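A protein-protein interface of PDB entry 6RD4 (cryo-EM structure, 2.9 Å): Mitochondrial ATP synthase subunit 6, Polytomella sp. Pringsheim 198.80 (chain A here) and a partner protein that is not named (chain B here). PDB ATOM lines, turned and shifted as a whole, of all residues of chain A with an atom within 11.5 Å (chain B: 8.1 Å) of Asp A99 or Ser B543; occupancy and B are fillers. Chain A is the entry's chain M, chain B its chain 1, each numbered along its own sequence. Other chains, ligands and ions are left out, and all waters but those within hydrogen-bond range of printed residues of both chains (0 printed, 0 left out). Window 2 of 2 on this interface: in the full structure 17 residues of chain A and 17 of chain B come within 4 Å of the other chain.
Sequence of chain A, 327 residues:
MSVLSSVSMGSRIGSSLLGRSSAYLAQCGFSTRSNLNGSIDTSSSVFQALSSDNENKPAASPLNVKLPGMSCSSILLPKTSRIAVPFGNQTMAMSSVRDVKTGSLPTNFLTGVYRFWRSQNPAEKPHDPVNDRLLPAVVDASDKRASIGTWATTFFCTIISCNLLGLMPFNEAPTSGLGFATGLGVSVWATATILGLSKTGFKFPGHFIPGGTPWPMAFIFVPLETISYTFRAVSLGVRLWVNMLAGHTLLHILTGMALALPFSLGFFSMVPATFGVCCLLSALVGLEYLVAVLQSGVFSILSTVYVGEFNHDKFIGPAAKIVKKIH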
ATOM      1  N   SER A  95     -32.004  15.471 -23.102  1.00  0.00           N
ATOM      2  CA  SER A  95     -33.317  16.102 -23.043  1.00  0.00           C
ATOM      3  C   SER A  95     -33.290  17.284 -22.077  1.00  0.00           C
ATOM      4  O   SER A  95     -34.065  18.232 -22.203  1.00  0.00           O
ATOM      5  CB  SER A  95     -34.378  15.082 -22.630  1.00  0.00           C
ATOM      6  OG  SER A  95     -34.356  13.960 -23.497  1.00  0.00           O
ATOM      7  N   SER A  96     -32.381  17.205 -21.113  1.00  0.00           N
ATOM      8  CA  SER A  96     -32.065  18.294 -20.202  1.00  0.00           C
ATOM      9  C   SER A  96     -30.677  18.792 -20.572  1.00  0.00           C
ATOM     10  O   SER A  96     -29.702  18.040 -20.491  1.00  0.00           O
ATOM     11  CB  SER A  96     -32.114  17.824 -18.752  1.00  0.00           C
ATOM     12  OG  SER A  96     -31.581  18.800 -17.876  1.00  0.00           O
ATOM     13  N   VAL A  97     -30.583  20.043 -20.984  1.00  0.00           N
ATOM     14  CA  VAL A  97     -29.298  20.572 -21.397  1.00  0.00           C
ATOM     15  C   VAL A  97     -28.499  20.998 -20.177  1.00  0.00           C
ATOM     16  O   VAL A  97     -29.022  21.154 -19.079  1.00  0.00           O
ATOM     17  CB  VAL A  97     -29.474  21.730 -22.378  1.00  0.00           C
ATOM     18  CG1 VAL A  97     -30.331  21.277 -23.492  1.00  0.00           C
ATOM     19  CG2 VAL A  97     -30.082  22.875 -21.688  1.00  0.00           C
ATOM     20  N   ARG A  98     -27.205  21.163 -20.377  1.00  0.00           N
ATOM     21  CA  ARG A  98     -26.361  21.524 -19.266  1.00  0.00           C
ATOM     22  C   ARG A  98     -26.447  23.012 -19.014  1.00  0.00           C
ATOM     23  O   ARG A  98     -26.941  23.778 -19.834  1.00  0.00           O
ATOM     24  CB  ARG A  98     -24.921  21.112 -19.523  1.00  0.00           C
ATOM     25  CG  ARG A  98     -24.199  21.946 -20.530  1.00  0.00           C
ATOM     26  CD  ARG A  98     -23.026  21.187 -21.068  1.00  0.00           C
ATOM     27  NE  ARG A  98     -23.418  19.845 -21.468  1.00  0.00           N
ATOM     28  CZ  ARG A  98     -22.567  18.907 -21.842  1.00  0.00           C
ATOM     29  NH1 ARG A  98     -21.278  19.165 -21.875  1.00  0.00           N
ATOM     30  NH2 ARG A  98     -23.010  17.716 -22.184  1.00  0.00           N
ATOM     31  N   ASP A  99     -25.973  23.414 -17.853  1.00  0.00           N
ATOM     32  CA  ASP A  99     -25.998  24.804 -17.443  1.00  0.00           C
ATOM     33  C   ASP A  99     -24.638  25.414 -17.673  1.00  0.00           C
ATOM     34  O   ASP A  99     -23.610  24.795 -17.403  1.00  0.00           O
ATOM     35  CB  ASP A  99     -26.378  24.937 -15.978  1.00  0.00           C
ATOM     36  CG  ASP A  99     -26.987  26.253 -15.670  1.00  0.00           C
ATOM     37  OD1 ASP A  99     -26.854  27.168 -16.477  1.00  0.00           O
ATOM     38  OD2 ASP A  99     -27.599  26.387 -14.609  1.00  0.00           O
ATOM     39  N   VAL A 100     -24.637  26.635 -18.168  1.00  0.00           N
ATOM     40  CA  VAL A 100     -23.425  27.320 -18.553  1.00  0.00           C
ATOM     41  C   VAL A 100     -23.277  28.516 -17.644  1.00  0.00           C
ATOM     42  O   VAL A 100     -24.245  29.236 -17.411  1.00  0.00           O
ATOM     43  CB  VAL A 100     -23.478  27.761 -20.019  1.00  0.00           C
ATOM     44  CG1 VAL A 100     -22.151  28.267 -20.438  1.00  0.00           C
ATOM     45  CG2 VAL A 100     -23.907  26.642 -20.876  1.00  0.00           C
ATOM     46  N   LYS A 101     -22.093  28.713 -17.112  1.00  0.00           N
ATOM     47  CA  LYS A 101     -21.801  29.956 -16.436  1.00  0.00           C
ATOM     48  C   LYS A 101     -21.607  31.043 -17.464  1.00  0.00           C
ATOM     49  O   LYS A 101     -20.990  30.816 -18.503  1.00  0.00           O
ATOM     50  CB  LYS A 101     -20.549  29.793 -15.611  1.00  0.00           C
ATOM     51  CG  LYS A 101     -20.128  30.990 -14.871  1.00  0.00           C
ATOM     52  CD  LYS A 101     -19.147  30.590 -13.856  1.00  0.00           C
ATOM     53  CE  LYS A 101     -17.871  30.249 -14.481  1.00  0.00           C
ATOM     54  NZ  LYS A 101     -17.161  31.491 -14.726  1.00  0.00           N
ATOM     55  N   THR A 102     -22.151  32.225 -17.205  1.00  0.00           N
ATOM     56  CA  THR A 102     -21.914  33.320 -18.124  1.00  0.00           C
ATOM     57  C   THR A 102     -20.500  33.813 -17.933  1.00  0.00           C
ATOM     58  O   THR A 102     -19.973  33.788 -16.828  1.00  0.00           O
ATOM     59  CB  THR A 102     -22.875  34.479 -17.912  1.00  0.00           C
ATOM     60  OG1 THR A 102     -22.732  34.967 -16.593  1.00  0.00           O
ATOM     61  CG2 THR A 102     -24.281  34.064 -18.131  1.00  0.00           C
ATOM     62  N   GLY A 103     -19.874  34.229 -19.021  1.00  0.00           N
ATOM     63  CA  GLY A 103     -18.545  34.774 -18.923  1.00  0.00           C
ATOM     64  C   GLY A 103     -17.479  33.752 -18.668  1.00  0.00           C
ATOM     65  O   GLY A 103     -16.454  34.080 -18.078  1.00  0.00           O
ATOM     66  N   SER A 104     -17.703  32.513 -19.084  1.00  0.00           N
ATOM     67  CA  SER A 104     -16.685  31.487 -19.038  1.00  0.00           C
ATOM     68  C   SER A 104     -15.581  31.829 -20.009  1.00  0.00           C
ATOM     69  O   SER A 104     -15.794  32.550 -20.969  1.00  0.00           O
ATOM     70  CB  SER A 104     -17.279  30.154 -19.428  1.00  0.00           C
ATOM     71  OG  SER A 104     -18.188  29.720 -18.465  1.00  0.00           O
ATOM     72  N   PRO A 106     -14.062  29.631 -22.214  1.00  0.00           N
ATOM     73  CA  PRO A 106     -14.338  29.152 -23.571  1.00  0.00           C
ATOM     74  C   PRO A 106     -15.454  29.887 -24.274  1.00  0.00           C
ATOM     75  O   PRO A 106     -15.498  29.883 -25.502  1.00  0.00           O
ATOM     76  CB  PRO A 106     -14.695  27.689 -23.344  1.00  0.00           C
ATOM     77  CG  PRO A 106     -14.027  27.356 -22.166  1.00  0.00           C
ATOM     78  CD  PRO A 106     -14.165  28.495 -21.288  1.00  0.00           C
ATOM     79  N   THR A 107     -16.368  30.496 -23.537  1.00  0.00           N
ATOM     80  CA  THR A 107     -17.412  31.313 -24.132  1.00  0.00           C
ATOM     81  C   THR A 107     -16.853  32.639 -24.597  1.00  0.00           C
ATOM     82  O   THR A 107     -17.296  33.187 -25.602  1.00  0.00           O
ATOM     83  CB  THR A 107     -18.515  31.513 -23.104  1.00  0.00           C
ATOM     84  OG1 THR A 107     -18.923  30.239 -22.613  1.00  0.00           O
ATOM     85  CG2 THR A 107     -19.706  32.193 -23.671  1.00  0.00           C
ATOM     86  N   ASP B 539     -20.534  34.943 -12.375  1.00  0.00           N
ATOM     87  CA  ASP B 539     -20.967  33.600 -12.030  1.00  0.00           C
ATOM     88  C   ASP B 539     -22.428  33.309 -12.312  1.00  0.00           C
ATOM     89  O   ASP B 539     -22.935  32.329 -11.777  1.00  0.00           O
ATOM     90  CB  ASP B 539     -20.683  33.271 -10.562  1.00  0.00           C
ATOM     91  CG  ASP B 539     -21.061  34.388  -9.606  1.00  0.00           C
ATOM     92  OD1 ASP B 539     -22.031  35.112  -9.850  1.00  0.00           O
ATOM     93  OD2 ASP B 539     -20.387  34.542  -8.577  1.00  0.00           O
ATOM     94  N   LEU B 540     -23.125  34.105 -13.086  1.00  0.00           N
ATOM     95  CA  LEU B 540     -24.550  33.879 -13.259  1.00  0.00           C
ATOM     96  C   LEU B 540     -24.756  32.692 -14.175  1.00  0.00           C
ATOM     97  O   LEU B 540     -24.149  32.643 -15.233  1.00  0.00           O
ATOM     98  CB  LEU B 540     -25.208  35.106 -13.856  1.00  0.00           C
ATOM     99  CG  LEU B 540     -26.704  35.324 -14.023  1.00  0.00           C
ATOM    100  CD1 LEU B 540     -27.399  35.299 -12.748  1.00  0.00           C
ATOM    101  CD2 LEU B 540     -26.864  36.629 -14.625  1.00  0.00           C
ATOM    102  N   PRO B 541     -25.556  31.710 -13.802  1.00  0.00           N
ATOM    103  CA  PRO B 541     -25.831  30.637 -14.735  1.00  0.00           C
ATOM    104  C   PRO B 541     -26.781  31.085 -15.819  1.00  0.00           C
ATOM    105  O   PRO B 541     -27.501  32.063 -15.693  1.00  0.00           O
ATOM    106  CB  PRO B 541     -26.451  29.556 -13.854  1.00  0.00           C
ATOM    107  CG  PRO B 541     -26.788  30.161 -12.680  1.00  0.00           C
ATOM    108  CD  PRO B 541     -25.956  31.325 -12.455  1.00  0.00           C
ATOM    109  N   HIS B 542     -26.754  30.361 -16.915  1.00  0.00           N
ATOM    110  CA  HIS B 542     -27.689  30.615 -17.985  1.00  0.00           C
ATOM    111  C   HIS B 542     -29.091  30.174 -17.656  1.00  0.00           C
ATOM    112  O   HIS B 542     -30.020  30.560 -18.360  1.00  0.00           O
ATOM    113  CB  HIS B 542     -27.233  29.900 -19.230  1.00  0.00           C
ATOM    114  CG  HIS B 542     -26.314  30.694 -20.085  1.00  0.00           C
ATOM    115  ND1 HIS B 542     -25.010  30.928 -19.742  1.00  0.00           N
ATOM    116  CD2 HIS B 542     -26.483  31.235 -21.304  1.00  0.00           C
ATOM    117  CE1 HIS B 542     -24.425  31.620 -20.694  1.00  0.00           C
ATOM    118  NE2 HIS B 542     -25.297  31.815 -21.655  1.00  0.00           N
ATOM    119  N   SER B 543     -29.265  29.349 -16.634  1.00  0.00           N
ATOM    120  CA  SER B 543     -30.597  28.919 -16.253  1.00  0.00           C
ATOM    121  C   SER B 543     -31.324  29.997 -15.500  1.00  0.00           C
ATOM    122  O   SER B 543     -32.550  30.041 -15.520  1.00  0.00           O
ATOM    123  CB  SER B 543     -30.508  27.686 -15.394  1.00  0.00           C
ATOM    124  OG  SER B 543     -29.439  27.815 -14.500  1.00  0.00           O
ATOM    125  N   VAL B 544     -30.582  30.847 -14.804  1.00  0.00           N
ATOM    126  CA  VAL B 544     -31.163  31.902 -14.000  1.00  0.00           C
ATOM    127  C   VAL B 544     -31.529  33.078 -14.868  1.00  0.00           C
ATOM    128  O   VAL B 544     -32.537  33.735 -14.627  1.00  0.00           O
ATOM    129  CB  VAL B 544     -30.185  32.259 -12.875  1.00  0.00           C
ATOM    130  CG1 VAL B 544     -30.586  33.461 -12.151  1.00  0.00           C
ATOM    131  CG2 VAL B 544     -30.190  31.167 -11.911  1.00  0.00           C
ATOM    132  N   VAL B 545     -30.762  33.327 -15.919  1.00  0.00           N
ATOM    133  CA  VAL B 545     -31.118  34.340 -16.904  1.00  0.00           C
ATOM    134  C   VAL B 545     -32.400  33.957 -17.615  1.00  0.00           C
ATOM    135  O   VAL B 545     -33.313  34.766 -17.764  1.00  0.00           O
ATOM    136  CB  VAL B 545     -29.976  34.514 -17.905  1.00  0.00           C
ATOM    137  CG1 VAL B 545     -30.399  35.382 -18.991  1.00  0.00           C
ATOM    138  CG2 VAL B 545     -28.813  35.068 -17.253  1.00  0.00           C
ATOM    139  N   ALA B 546     -32.498  32.714 -18.050  1.00  0.00           N
ATOM    140  CA  ALA B 546     -33.689  32.267 -18.744  1.00  0.00           C
ATOM    141  C   ALA B 546     -34.854  32.072 -17.815  1.00  0.00           C
ATOM    142  O   ALA B 546     -35.978  31.912 -18.282  1.00  0.00           O
ATOM    143  CB  ALA B 546     -33.402  30.972 -19.474  1.00  0.00           C
ATOM    144  N   HIS B 547     -34.612  32.023 -16.515  1.00  0.00           N
ATOM    145  CA  HIS B 547     -35.705  32.033 -15.567  1.00  0.00           C
ATOM    146  C   HIS B 547     -36.212  33.440 -15.373  1.00  0.00           C
ATOM    147  O   HIS B 547     -37.403  33.698 -15.512  1.00  0.00           O
ATOM    148  CB  HIS B 547     -35.255  31.463 -14.237  1.00  0.00           C
ATOM    149  CG  HIS B 547     -36.341  31.422 -13.222  1.00  0.00           C
ATOM    150  ND1 HIS B 547     -36.399  32.286 -12.158  1.00  0.00           N
ATOM    151  CD2 HIS B 547     -37.434  30.638 -13.132  1.00  0.00           C
ATOM    152  CE1 HIS B 547     -37.477  32.030 -11.447  1.00  0.00           C
ATOM    153  NE2 HIS B 547     -38.127  31.037 -12.020  1.00  0.00           N
ATOM    154  N   MET B 548     -35.302  34.358 -15.080  1.00  0.00           N
ATOM    155  CA  MET B 548     -35.652  35.739 -14.818  1.00  0.00           C
ATOM    156  C   MET B 548     -36.210  36.412 -16.050  1.00  0.00           C
ATOM    157  O   MET B 548     -37.224  37.102 -15.979  1.00  0.00           O
ATOM    158  CB  MET B 548     -34.429  36.488 -14.341  1.00  0.00           C
ATOM    159  CG  MET B 548     -34.163  36.396 -12.924  1.00  0.00           C
ATOM    160  SD  MET B 548     -33.071  37.723 -12.552  1.00  0.00           S
ATOM    161  CE  MET B 548     -31.561  36.938 -12.928  1.00  0.00           C
ATOM    162  N   ASP B 549     -35.577  36.227 -17.193  1.00  0.00           N
ATOM    163  CA  ASP B 549     -35.998  36.881 -18.422  1.00  0.00           C
ATOM    164  C   ASP B 549     -36.263  35.818 -19.469  1.00  0.00           C
ATOM    165  O   ASP B 549     -35.389  35.512 -20.281  1.00  0.00           O
ATOM    166  CB  ASP B 549     -34.950  37.868 -18.902  1.00  0.00           C
ATOM    167  CG  ASP B 549     -35.567  39.092 -19.487  1.00  0.00           C
ATOM    168  OD1 ASP B 549     -36.792  39.094 -19.642  1.00  0.00           O
ATOM    169  OD2 ASP B 549     -34.852  40.078 -19.731  1.00  0.00           O
ATOM    170  N   ILE B 553     -34.590  35.574 -23.698  1.00  0.00           N
ATOM    171  CA  ILE B 553     -33.981  34.354 -24.189  1.00  0.00           C
ATOM    172  C   ILE B 553     -34.770  33.786 -25.350  1.00  0.00           C
ATOM    173  O   ILE B 553     -34.190  33.265 -26.292  1.00  0.00           O
ATOM    174  CB  ILE B 553     -33.870  33.386 -23.006  1.00  0.00           C
ATOM    175  CG1 ILE B 553     -32.903  33.946 -21.980  1.00  0.00           C
ATOM    176  CG2 ILE B 553     -33.483  32.036 -23.409  1.00  0.00           C
ATOM    177  CD1 ILE B 553     -31.581  34.289 -22.511  1.00  0.00           C
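The side-chain carboxylate (OD1) of Asp A99 sits at hydrogen-bond distance from the backbone NH (N) of His B542.
The side-chain carboxylate (OD1) of Asp A99 lies within hydrogen-bond range of the backbone NH (N) of Ser B543, at 3.3 Å.
The backbone NH (N) of His B542 lies within hydrogen-bond range of the backbone carbonyl oxygen (O) of Val A100 (2.8 Å).
The backbone NH (N) of Thr A102 is in hydrogen-bond range of the backbone carbonyl oxygen (O) of Leu B540, 2.8 Å away.
OG of Ser A104 lies within hydrogen-bond range of O of Lys A101 (3.0 Å).
Among the printed residues, merely in contact across the chains: Val A100 with Pro B541 (3.4 Å), Asp A99 with Pro B541 (3.5 Å), Thr A102 with His B542 (3.5 Å), Lys A101 with Leu B540 (3.7 Å) and Lys A101 with Asp B539 (3.9 Å).
Of the printed residues of chain B, Asp A99 touches Pro B541, His B542 and Ser B543.
Pro B541 touches two residues of chain A.
His B542 touches just these residues of chain A: Asp A99 (3.2 Å), Val A100 (2.8 Å) and Thr A102 (3.5 Å).
No residue of chain A comes within 4 Å of Val B544.
No residue of chain A comes within 4 Å of Val B545.
Ala B546 touches none of the printed residues of chain A.
No residue of chain A comes within 4 Å of His B547.
Of the printed residues of chain B, Lys A101 touches Asp B539 (3.9 Å) and Leu B540 (3.7 Å).
Of the printed residues of chain A, Leu B540 touches Lys A101 and Thr A102.
Of the printed residues of chain B, Val A100 touches Pro B541 (3.4 Å) and His B542 (2.8 Å).
Met B548 touches none of the printed residues of chain A.
Thr A107 touches none of the printed residues of chain B.
The nearest printed residue of chain A that does not touch Leu B540 is Val A100 (4.04 Å).
Printed residues of chain A that touch a printed residue of chain B: Asp A99, Val A100, Lys A101 and Thr A102.
Hydrophobic or aromatic side chains of chain A that line the printed part of chain B: Val A100.
Among the printed residues, 9 pairs touch across the chains.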
